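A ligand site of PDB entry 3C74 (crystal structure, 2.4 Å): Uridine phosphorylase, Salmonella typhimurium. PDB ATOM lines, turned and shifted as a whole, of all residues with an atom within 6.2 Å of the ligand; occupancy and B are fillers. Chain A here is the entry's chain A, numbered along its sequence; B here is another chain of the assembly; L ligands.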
ATOM      1  N   GLY A  26     -15.706  -4.284  25.827  1.00  0.00           N
ATOM      2  CA  GLY A  26     -15.642  -5.532  25.083  1.00  0.00           C
ATOM      3  C   GLY A  26     -14.509  -6.441  25.519  1.00  0.00           C
ATOM      4  O   GLY A  26     -14.677  -7.656  25.634  1.00  0.00           O
ATOM      5  N   GLY A  68     -17.133  -9.263  25.550  1.00  0.00           N
ATOM      6  CA  GLY A  68     -16.535  -9.942  24.396  1.00  0.00           C
ATOM      7  C   GLY A  68     -16.959  -9.255  23.110  1.00  0.00           C
ATOM      8  O   GLY A  68     -17.546  -8.171  23.125  1.00  0.00           O
ATOM      9  N   ILE A  69     -16.667  -9.901  21.983  1.00  0.00           N
ATOM     10  CA  ILE A  69     -17.059  -9.370  20.669  1.00  0.00           C
ATOM     11  C   ILE A  69     -18.430  -9.925  20.275  1.00  0.00           C
ATOM     12  O   ILE A  69     -18.677 -11.130  20.362  1.00  0.00           O
ATOM     13  CB  ILE A  69     -16.006  -9.696  19.572  1.00  0.00           C
ATOM     14  CG1 ILE A  69     -14.677  -9.000  19.902  1.00  0.00           C
ATOM     15  CG2 ILE A  69     -16.507  -9.275  18.187  1.00  0.00           C
ATOM     16  CD1 ILE A  69     -13.465  -9.613  19.218  1.00  0.00           C
ATOM     17  N   GLY A  70     -19.330  -9.025  19.860  1.00  0.00           N
ATOM     18  CA  GLY A  70     -20.613  -9.411  19.298  1.00  0.00           C
ATOM     19  C   GLY A  70     -21.829  -9.236  20.192  1.00  0.00           C
ATOM     20  O   GLY A  70     -21.727  -9.296  21.422  1.00  0.00           O
ATOM     21  N   ARG A  91     -21.676   1.378  27.640  1.00  0.00           N
ATOM     22  CA  ARG A  91     -20.638   0.753  26.825  1.00  0.00           C
ATOM     23  C   ARG A  91     -19.562   1.744  26.419  1.00  0.00           C
ATOM     24  O   ARG A  91     -19.852   2.871  25.991  1.00  0.00           O
ATOM     25  CB  ARG A  91     -21.210   0.073  25.581  1.00  0.00           C
ATOM     26  CG  ARG A  91     -20.128  -0.509  24.672  1.00  0.00           C
ATOM     27  CD  ARG A  91     -20.651  -1.577  23.734  1.00  0.00           C
ATOM     28  NE  ARG A  91     -19.573  -2.284  23.045  1.00  0.00           N
ATOM     29  CZ  ARG A  91     -18.892  -3.318  23.558  1.00  0.00           C
ATOM     30  NH1 ARG A  91     -19.168  -3.783  24.767  1.00  0.00           N
ATOM     31  NH2 ARG A  91     -17.927  -3.889  22.843  1.00  0.00           N
ATOM     32  N   GLY A  93     -16.133   1.483  23.881  1.00  0.00           N
ATOM     33  CA  GLY A  93     -15.543   0.618  22.867  1.00  0.00           C
ATOM     34  C   GLY A  93     -14.555   1.317  21.941  1.00  0.00           C
ATOM     35  O   GLY A  93     -14.133   2.442  22.207  1.00  0.00           O
ATOM     36  N   THR A  94     -14.180   0.621  20.867  1.00  0.00           N
ATOM     37  CA  THR A  94     -13.303   1.165  19.825  1.00  0.00           C
ATOM     38  C   THR A  94     -14.016   1.036  18.481  1.00  0.00           C
ATOM     39  O   THR A  94     -14.840   0.140  18.290  1.00  0.00           O
ATOM     40  CB  THR A  94     -11.938   0.460  19.771  1.00  0.00           C
ATOM     41  OG1 THR A  94     -12.103  -0.943  19.513  1.00  0.00           O
ATOM     42  CG2 THR A  94     -11.170   0.656  21.078  1.00  0.00           C
ATOM     43  N   THR A  95     -13.689   1.931  17.547  1.00  0.00           N
ATOM     44  CA  THR A  95     -14.477   2.050  16.314  1.00  0.00           C
ATOM     45  C   THR A  95     -13.699   2.565  15.098  1.00  0.00           C
ATOM     46  O   THR A  95     -12.698   3.282  15.240  1.00  0.00           O
ATOM     47  CB  THR A  95     -15.749   2.921  16.554  1.00  0.00           C
ATOM     48  OG1 THR A  95     -16.582   2.880  15.392  1.00  0.00           O
ATOM     49  CG2 THR A  95     -15.389   4.371  16.893  1.00  0.00           C
ATOM     50  N   GLY A  96     -14.177   2.192  13.916  1.00  0.00           N
ATOM     51  CA  GLY A  96     -13.635   2.685  12.651  1.00  0.00           C
ATOM     52  C   GLY A  96     -14.547   3.725  12.038  1.00  0.00           C
ATOM     53  O   GLY A  96     -15.663   3.411  11.612  1.00  0.00           O
ATOM     54  N   PHE A 162     -17.029  -8.279  11.183  1.00  0.00           N
ATOM     55  CA  PHE A 162     -15.931  -7.348  11.015  1.00  0.00           C
ATOM     56  C   PHE A 162     -15.658  -7.048   9.542  1.00  0.00           C
ATOM     57  O   PHE A 162     -15.387  -5.901   9.176  1.00  0.00           O
ATOM     58  CB  PHE A 162     -14.663  -7.901  11.679  1.00  0.00           C
ATOM     59  CG  PHE A 162     -13.531  -6.922  11.762  1.00  0.00           C
ATOM     60  CD1 PHE A 162     -13.474  -5.996  12.812  1.00  0.00           C
ATOM     61  CD2 PHE A 162     -12.514  -6.921  10.808  1.00  0.00           C
ATOM     62  CE1 PHE A 162     -12.427  -5.082  12.899  1.00  0.00           C
ATOM     63  CE2 PHE A 162     -11.461  -6.003  10.887  1.00  0.00           C
ATOM     64  CZ  PHE A 162     -11.417  -5.091  11.924  1.00  0.00           C
ATOM     65  N   GLN A 166     -18.933  -4.706   7.026  1.00  0.00           N
ATOM     66  CA  GLN A 166     -18.312  -3.383   7.010  1.00  0.00           C
ATOM     67  C   GLN A 166     -17.698  -3.093   5.637  1.00  0.00           C
ATOM     68  O   GLN A 166     -16.911  -2.153   5.481  1.00  0.00           O
ATOM     69  CB  GLN A 166     -17.255  -3.263   8.105  1.00  0.00           C
ATOM     70  CG  GLN A 166     -17.800  -3.423   9.529  1.00  0.00           C
ATOM     71  CD  GLN A 166     -16.794  -3.067  10.605  1.00  0.00           C
ATOM     72  OE1 GLN A 166     -15.900  -2.238  10.391  1.00  0.00           O
ATOM     73  NE2 GLN A 166     -16.920  -3.693  11.766  1.00  0.00           N
ATOM     74  N   ARG A 168     -15.446  -4.815   3.749  1.00  0.00           N
ATOM     75  CA  ARG A 168     -14.018  -5.036   3.586  1.00  0.00           C
ATOM     76  C   ARG A 168     -13.750  -6.072   2.491  1.00  0.00           C
ATOM     77  O   ARG A 168     -14.364  -7.147   2.483  1.00  0.00           O
ATOM     78  CB  ARG A 168     -13.371  -5.455   4.907  1.00  0.00           C
ATOM     79  CG  ARG A 168     -13.179  -4.305   5.900  1.00  0.00           C
ATOM     80  CD  ARG A 168     -12.481  -4.759   7.179  1.00  0.00           C
ATOM     81  NE  ARG A 168     -12.011  -3.622   7.977  1.00  0.00           N
ATOM     82  CZ  ARG A 168     -12.625  -3.141   9.053  1.00  0.00           C
ATOM     83  NH1 ARG A 168     -13.750  -3.678   9.490  1.00  0.00           N
ATOM     84  NH2 ARG A 168     -12.102  -2.102   9.693  1.00  0.00           N
ATOM     85  N   TYR A 195     -18.436   2.322  12.131  1.00  0.00           N
ATOM     86  CA  TYR A 195     -18.749   0.917  12.286  1.00  0.00           C
ATOM     87  C   TYR A 195     -18.309   0.413  13.657  1.00  0.00           C
ATOM     88  O   TYR A 195     -17.223   0.742  14.131  1.00  0.00           O
ATOM     89  CB  TYR A 195     -18.047   0.070  11.216  1.00  0.00           C
ATOM     90  CG  TYR A 195     -18.651   0.082   9.827  1.00  0.00           C
ATOM     91  CD1 TYR A 195     -19.933  -0.440   9.586  1.00  0.00           C
ATOM     92  CD2 TYR A 195     -17.923   0.558   8.740  1.00  0.00           C
ATOM     93  CE1 TYR A 195     -20.476  -0.453   8.295  1.00  0.00           C
ATOM     94  CE2 TYR A 195     -18.463   0.554   7.454  1.00  0.00           C
ATOM     95  CZ  TYR A 195     -19.737   0.050   7.240  1.00  0.00           C
ATOM     96  OH  TYR A 195     -20.240   0.048   5.956  1.00  0.00           O
ATOM     97  N   GLU A 196     -19.175  -0.374  14.297  1.00  0.00           N
ATOM     98  CA  GLU A 196     -18.790  -1.249  15.414  1.00  0.00           C
ATOM     99  C   GLU A 196     -19.673  -2.513  15.396  1.00  0.00           C
ATOM    100  O   GLU A 196     -20.361  -2.754  14.400  1.00  0.00           O
ATOM    101  CB  GLU A 196     -18.772  -0.526  16.770  1.00  0.00           C
ATOM    102  CG  GLU A 196     -20.078   0.137  17.200  1.00  0.00           C
ATOM    103  CD  GLU A 196     -21.025  -0.825  17.893  1.00  0.00           C
ATOM    104  OE1 GLU A 196     -20.728  -1.258  19.034  1.00  0.00           O
ATOM    105  OE2 GLU A 196     -22.074  -1.145  17.306  1.00  0.00           O
ATOM    106  N   MET A 197     -19.654  -3.308  16.463  1.00  0.00           N
ATOM    107  CA  MET A 197     -20.250  -4.646  16.414  1.00  0.00           C
ATOM    108  C   MET A 197     -21.184  -5.036  17.580  1.00  0.00           C
ATOM    109  O   MET A 197     -21.571  -6.206  17.685  1.00  0.00           O
ATOM    110  CB  MET A 197     -19.151  -5.705  16.246  1.00  0.00           C
ATOM    111  CG  MET A 197     -18.397  -5.641  14.922  1.00  0.00           C
ATOM    112  SD  MET A 197     -17.047  -6.842  14.773  1.00  0.00           S
ATOM    113  CE  MET A 197     -17.952  -8.374  14.617  1.00  0.00           C
ATOM    114  N   GLU A 198     -21.552  -4.088  18.438  1.00  0.00           N
ATOM    115  CA  GLU A 198     -22.296  -4.432  19.670  1.00  0.00           C
ATOM    116  C   GLU A 198     -23.471  -3.531  20.043  1.00  0.00           C
ATOM    117  O   GLU A 198     -24.370  -3.964  20.778  1.00  0.00           O
ATOM    118  CB  GLU A 198     -21.345  -4.526  20.875  1.00  0.00           C
ATOM    119  CG  GLU A 198     -20.381  -5.707  20.872  1.00  0.00           C
ATOM    120  CD  GLU A 198     -19.118  -5.448  20.044  1.00  0.00           C
ATOM    121  OE1 GLU A 198     -18.791  -4.272  19.769  1.00  0.00           O
ATOM    122  OE2 GLU A 198     -18.460  -6.429  19.655  1.00  0.00           O
ATOM    123  N   ILE A 220     -10.187   4.471  16.272  1.00  0.00           N
ATOM    124  CA  ILE A 220      -8.860   3.848  16.133  1.00  0.00           C
ATOM    125  C   ILE A 220      -8.381   3.758  14.678  1.00  0.00           C
ATOM    126  O   ILE A 220      -7.192   3.531  14.418  1.00  0.00           O
ATOM    127  CB  ILE A 220      -8.779   2.462  16.851  1.00  0.00           C
ATOM    128  CG1 ILE A 220      -9.858   1.495  16.356  1.00  0.00           C
ATOM    129  CG2 ILE A 220      -8.863   2.626  18.361  1.00  0.00           C
ATOM    130  CD1 ILE A 220      -9.352   0.413  15.428  1.00  0.00           C
ATOM    131  N   VAL A 221      -9.315   3.961  13.749  1.00  0.00           N
ATOM    132  CA  VAL A 221      -9.021   3.908  12.306  1.00  0.00           C
ATOM    133  C   VAL A 221     -10.065   4.716  11.517  1.00  0.00           C
ATOM    134  O   VAL A 221     -11.209   4.844  11.951  1.00  0.00           O
ATOM    135  CB  VAL A 221      -8.909   2.425  11.787  1.00  0.00           C
ATOM    136  CG1 VAL A 221     -10.225   1.674  11.936  1.00  0.00           C
ATOM    137  CG2 VAL A 221      -8.395   2.367  10.344  1.00  0.00           C
ATOM    138  N   ARG A 223     -11.820   4.763   7.716  1.00  0.00           N
ATOM    139  CA  ARG A 223     -12.040   3.892   6.557  1.00  0.00           C
ATOM    140  C   ARG A 223     -11.872   4.559   5.184  1.00  0.00           C
ATOM    141  O   ARG A 223     -11.811   3.868   4.170  1.00  0.00           O
ATOM    142  CB  ARG A 223     -13.413   3.205   6.639  1.00  0.00           C
ATOM    143  CG  ARG A 223     -13.525   2.128   7.718  1.00  0.00           C
ATOM    144  CD  ARG A 223     -12.711   0.872   7.395  1.00  0.00           C
ATOM    145  NE  ARG A 223     -13.028   0.302   6.080  1.00  0.00           N
ATOM    146  CZ  ARG A 223     -14.043  -0.533   5.841  1.00  0.00           C
ATOM    147  NH1 ARG A 223     -14.851  -0.914   6.817  1.00  0.00           N
ATOM    148  NH2 ARG A 223     -14.241  -0.989   4.607  1.00  0.00           N
ATOM    149  N   GLU A 227      -8.491  -0.001   5.348  1.00  0.00           N
ATOM    150  CA  GLU A 227      -9.422  -0.985   5.888  1.00  0.00           C
ATOM    151  C   GLU A 227      -9.069  -1.385   7.317  1.00  0.00           C
ATOM    152  O   GLU A 227      -9.951  -1.635   8.137  1.00  0.00           O
ATOM    153  CB  GLU A 227      -9.472  -2.239   4.996  1.00  0.00           C
ATOM    154  CG  GLU A 227     -10.393  -2.138   3.789  1.00  0.00           C
ATOM    155  CD  GLU A 227     -10.648  -3.478   3.089  1.00  0.00           C
ATOM    156  OE1 GLU A 227     -11.235  -3.468   1.983  1.00  0.00           O
ATOM    157  OE2 GLU A 227     -10.274  -4.534   3.646  1.00  0.00           O
ATOM    158  N   PHE B   7      -5.401  -9.495  12.040  1.00  0.00           N
ATOM    159  CA  PHE B   7      -5.699  -8.409  12.978  1.00  0.00           C
ATOM    160  C   PHE B   7      -6.116  -8.852  14.392  1.00  0.00           C
ATOM    161  O   PHE B   7      -5.842  -8.132  15.360  1.00  0.00           O
ATOM    162  CB  PHE B   7      -6.730  -7.442  12.378  1.00  0.00           C
ATOM    163  CG  PHE B   7      -6.950  -6.203  13.201  1.00  0.00           C
ATOM    164  CD1 PHE B   7      -5.916  -5.276  13.374  1.00  0.00           C
ATOM    165  CD2 PHE B   7      -8.172  -5.949  13.798  1.00  0.00           C
ATOM    166  CE1 PHE B   7      -6.115  -4.124  14.137  1.00  0.00           C
ATOM    167  CE2 PHE B   7      -8.387  -4.805  14.559  1.00  0.00           C
ATOM    168  CZ  PHE B   7      -7.355  -3.887  14.728  1.00  0.00           C
ATOM    169  N   HIS B   8      -6.770 -10.000  14.507  1.00  0.00           N
ATOM    170  CA  HIS B   8      -7.292 -10.446  15.806  1.00  0.00           C
ATOM    171  C   HIS B   8      -6.546 -11.614  16.442  1.00  0.00           C
ATOM    172  O   HIS B   8      -6.254 -11.597  17.645  1.00  0.00           O
ATOM    173  CB  HIS B   8      -8.781 -10.785  15.699  1.00  0.00           C
ATOM    174  CG  HIS B   8      -9.654  -9.600  15.431  1.00  0.00           C
ATOM    175  ND1 HIS B   8      -9.996  -9.196  14.155  1.00  0.00           N
ATOM    176  CD2 HIS B   8     -10.261  -8.724  16.269  1.00  0.00           C
ATOM    177  CE1 HIS B   8     -10.775  -8.136  14.230  1.00  0.00           C
ATOM    178  NE2 HIS B   8     -10.946  -7.826  15.502  1.00  0.00           N
ATOM    179  N   ARG B  48      -8.013 -11.814  23.334  1.00  0.00           N
ATOM    180  CA  ARG B  48      -9.445 -11.762  23.671  1.00  0.00           C
ATOM    181  C   ARG B  48     -10.000 -13.169  23.909  1.00  0.00           C
ATOM    182  O   ARG B  48      -9.605 -13.810  24.882  1.00  0.00           O
ATOM    183  CB  ARG B  48     -10.232 -10.942  22.631  1.00  0.00           C
ATOM    184  CG  ARG B  48      -9.760  -9.499  22.569  1.00  0.00           C
ATOM    185  CD  ARG B  48     -10.551  -8.653  21.589  1.00  0.00           C
ATOM    186  NE  ARG B  48     -11.833  -8.220  22.124  1.00  0.00           N
ATOM    187  CZ  ARG B  48     -12.406  -7.049  21.860  1.00  0.00           C
ATOM    188  NH1 ARG B  48     -11.811  -6.176  21.059  1.00  0.00           N
ATOM    189  NH2 ARG B  48     -13.580  -6.754  22.405  1.00  0.00           N
ATOM    190  N   ILE B  76     -14.892 -13.841  12.681  1.00  0.00           N
ATOM    191  CA  ILE B  76     -13.523 -13.305  12.741  1.00  0.00           C
ATOM    192  C   ILE B  76     -12.490 -14.445  12.740  1.00  0.00           C
ATOM    193  O   ILE B  76     -11.546 -14.426  11.949  1.00  0.00           O
ATOM    194  CB  ILE B  76     -13.309 -12.379  13.970  1.00  0.00           C
ATOM    195  CG1 ILE B  76     -14.039 -11.052  13.787  1.00  0.00           C
ATOM    196  CG2 ILE B  76     -11.824 -12.152  14.212  1.00  0.00           C
ATOM    197  CD1 ILE B  76     -14.137 -10.189  15.051  1.00  0.00           C
HETATM  198  O1  LIG L   1     -16.068  -5.557  19.098  1.00  0.00           O
HETATM  199  C1  LIG L   1     -15.292  -5.150  17.967  1.00  0.00           C
HETATM  200  C2  LIG L   1     -15.711  -3.767  17.497  1.00  0.00           C
HETATM  201  O2  LIG L   1     -15.919  -3.762  16.079  1.00  0.00           O
HETATM  202  C3  LIG L   1     -15.406  -2.504  15.646  1.00  0.00           C
HETATM  203  N1  LIG L   1     -15.201  -2.154  14.236  1.00  0.00           N
HETATM  204  C4  LIG L   1     -14.029  -1.612  13.834  1.00  0.00           C
HETATM  205  O3  LIG L   1     -13.910  -1.277  12.629  1.00  0.00           O
HETATM  206  C5  LIG L   1     -12.960  -1.450  14.708  1.00  0.00           C
HETATM  207  C6  LIG L   1     -13.075  -1.831  16.054  1.00  0.00           C
HETATM  208  N2  LIG L   1     -14.243  -2.334  16.488  1.00  0.00           N
HETATM  209  C7  LIG L   1     -14.553  -2.815  17.821  1.00  0.00           C
HETATM  210  O4  LIG L   1     -13.477  -3.629  18.320  1.00  0.00           O
HETATM  211  C8  LIG L   1     -13.837  -5.012  18.396  1.00  0.00           C
HETATM  212  C9  LIG L   1     -12.914  -5.892  17.539  1.00  0.00           C
HETATM  213  O5  LIG L   1     -12.771  -5.396  16.208  1.00  0.00           O
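The side-chain carboxylate (OE2) of Glu 198 sits at hydrogen-bond distance from an oxygen (O1) of the ligand (2.6 Å). O4 of the ligand is in hydrogen-bond range of OG1 of Thr 94, at 3.2 Å. NE2 of His 8 of chain B is in hydrogen-bond range of O5 of the ligand. OE1 of Gln 166 sits close to O3 of the ligand (3.1 Å).
The backbone NH (N) of Glu 198 sits at hydrogen-bond distance from the side-chain carboxylate (OE1) of Glu 196, at 3.0 Å. The guanidinium group (NH2) of Arg 91 lies within salt-bridge range of the side-chain carboxylate (OE1) of Glu 198 (3.2 Å). The backbone NH of Gly 70 sits at hydrogen-bond distance from the side-chain carboxylate of Glu 198, at 2.7 Å. The side-chain amide oxygen (OE1) of Gln 166 sits at hydrogen-bond distance from the guanidinium group (NH1) of Arg 168, 2.7 Å away. O of Gln 166 sits at hydrogen-bond distance from NH1 of Arg 223. The backbone NH of Tyr 195 lies within hydrogen-bond range of the backbone carbonyl oxygen of Gly 96 (3.0 Å). The backbone carbonyl oxygen of Tyr 195 sits at hydrogen-bond distance from the side-chain hydroxyl of Thr 95. The backbone carbonyl oxygen (O) of Glu 227 sits at hydrogen-bond distance from the guanidinium group (NH2) of Arg 168 (2.7 Å).
An oxygen (O2) of the ligand lies close to the side-chain sulfur (SD) of Met 197, 3.5 Å away. Residues that only touch the ligand: Ile 69, Gly 96, Phe 162, Arg 168, Tyr 195, Glu 196 and Arg 48 of chain B.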
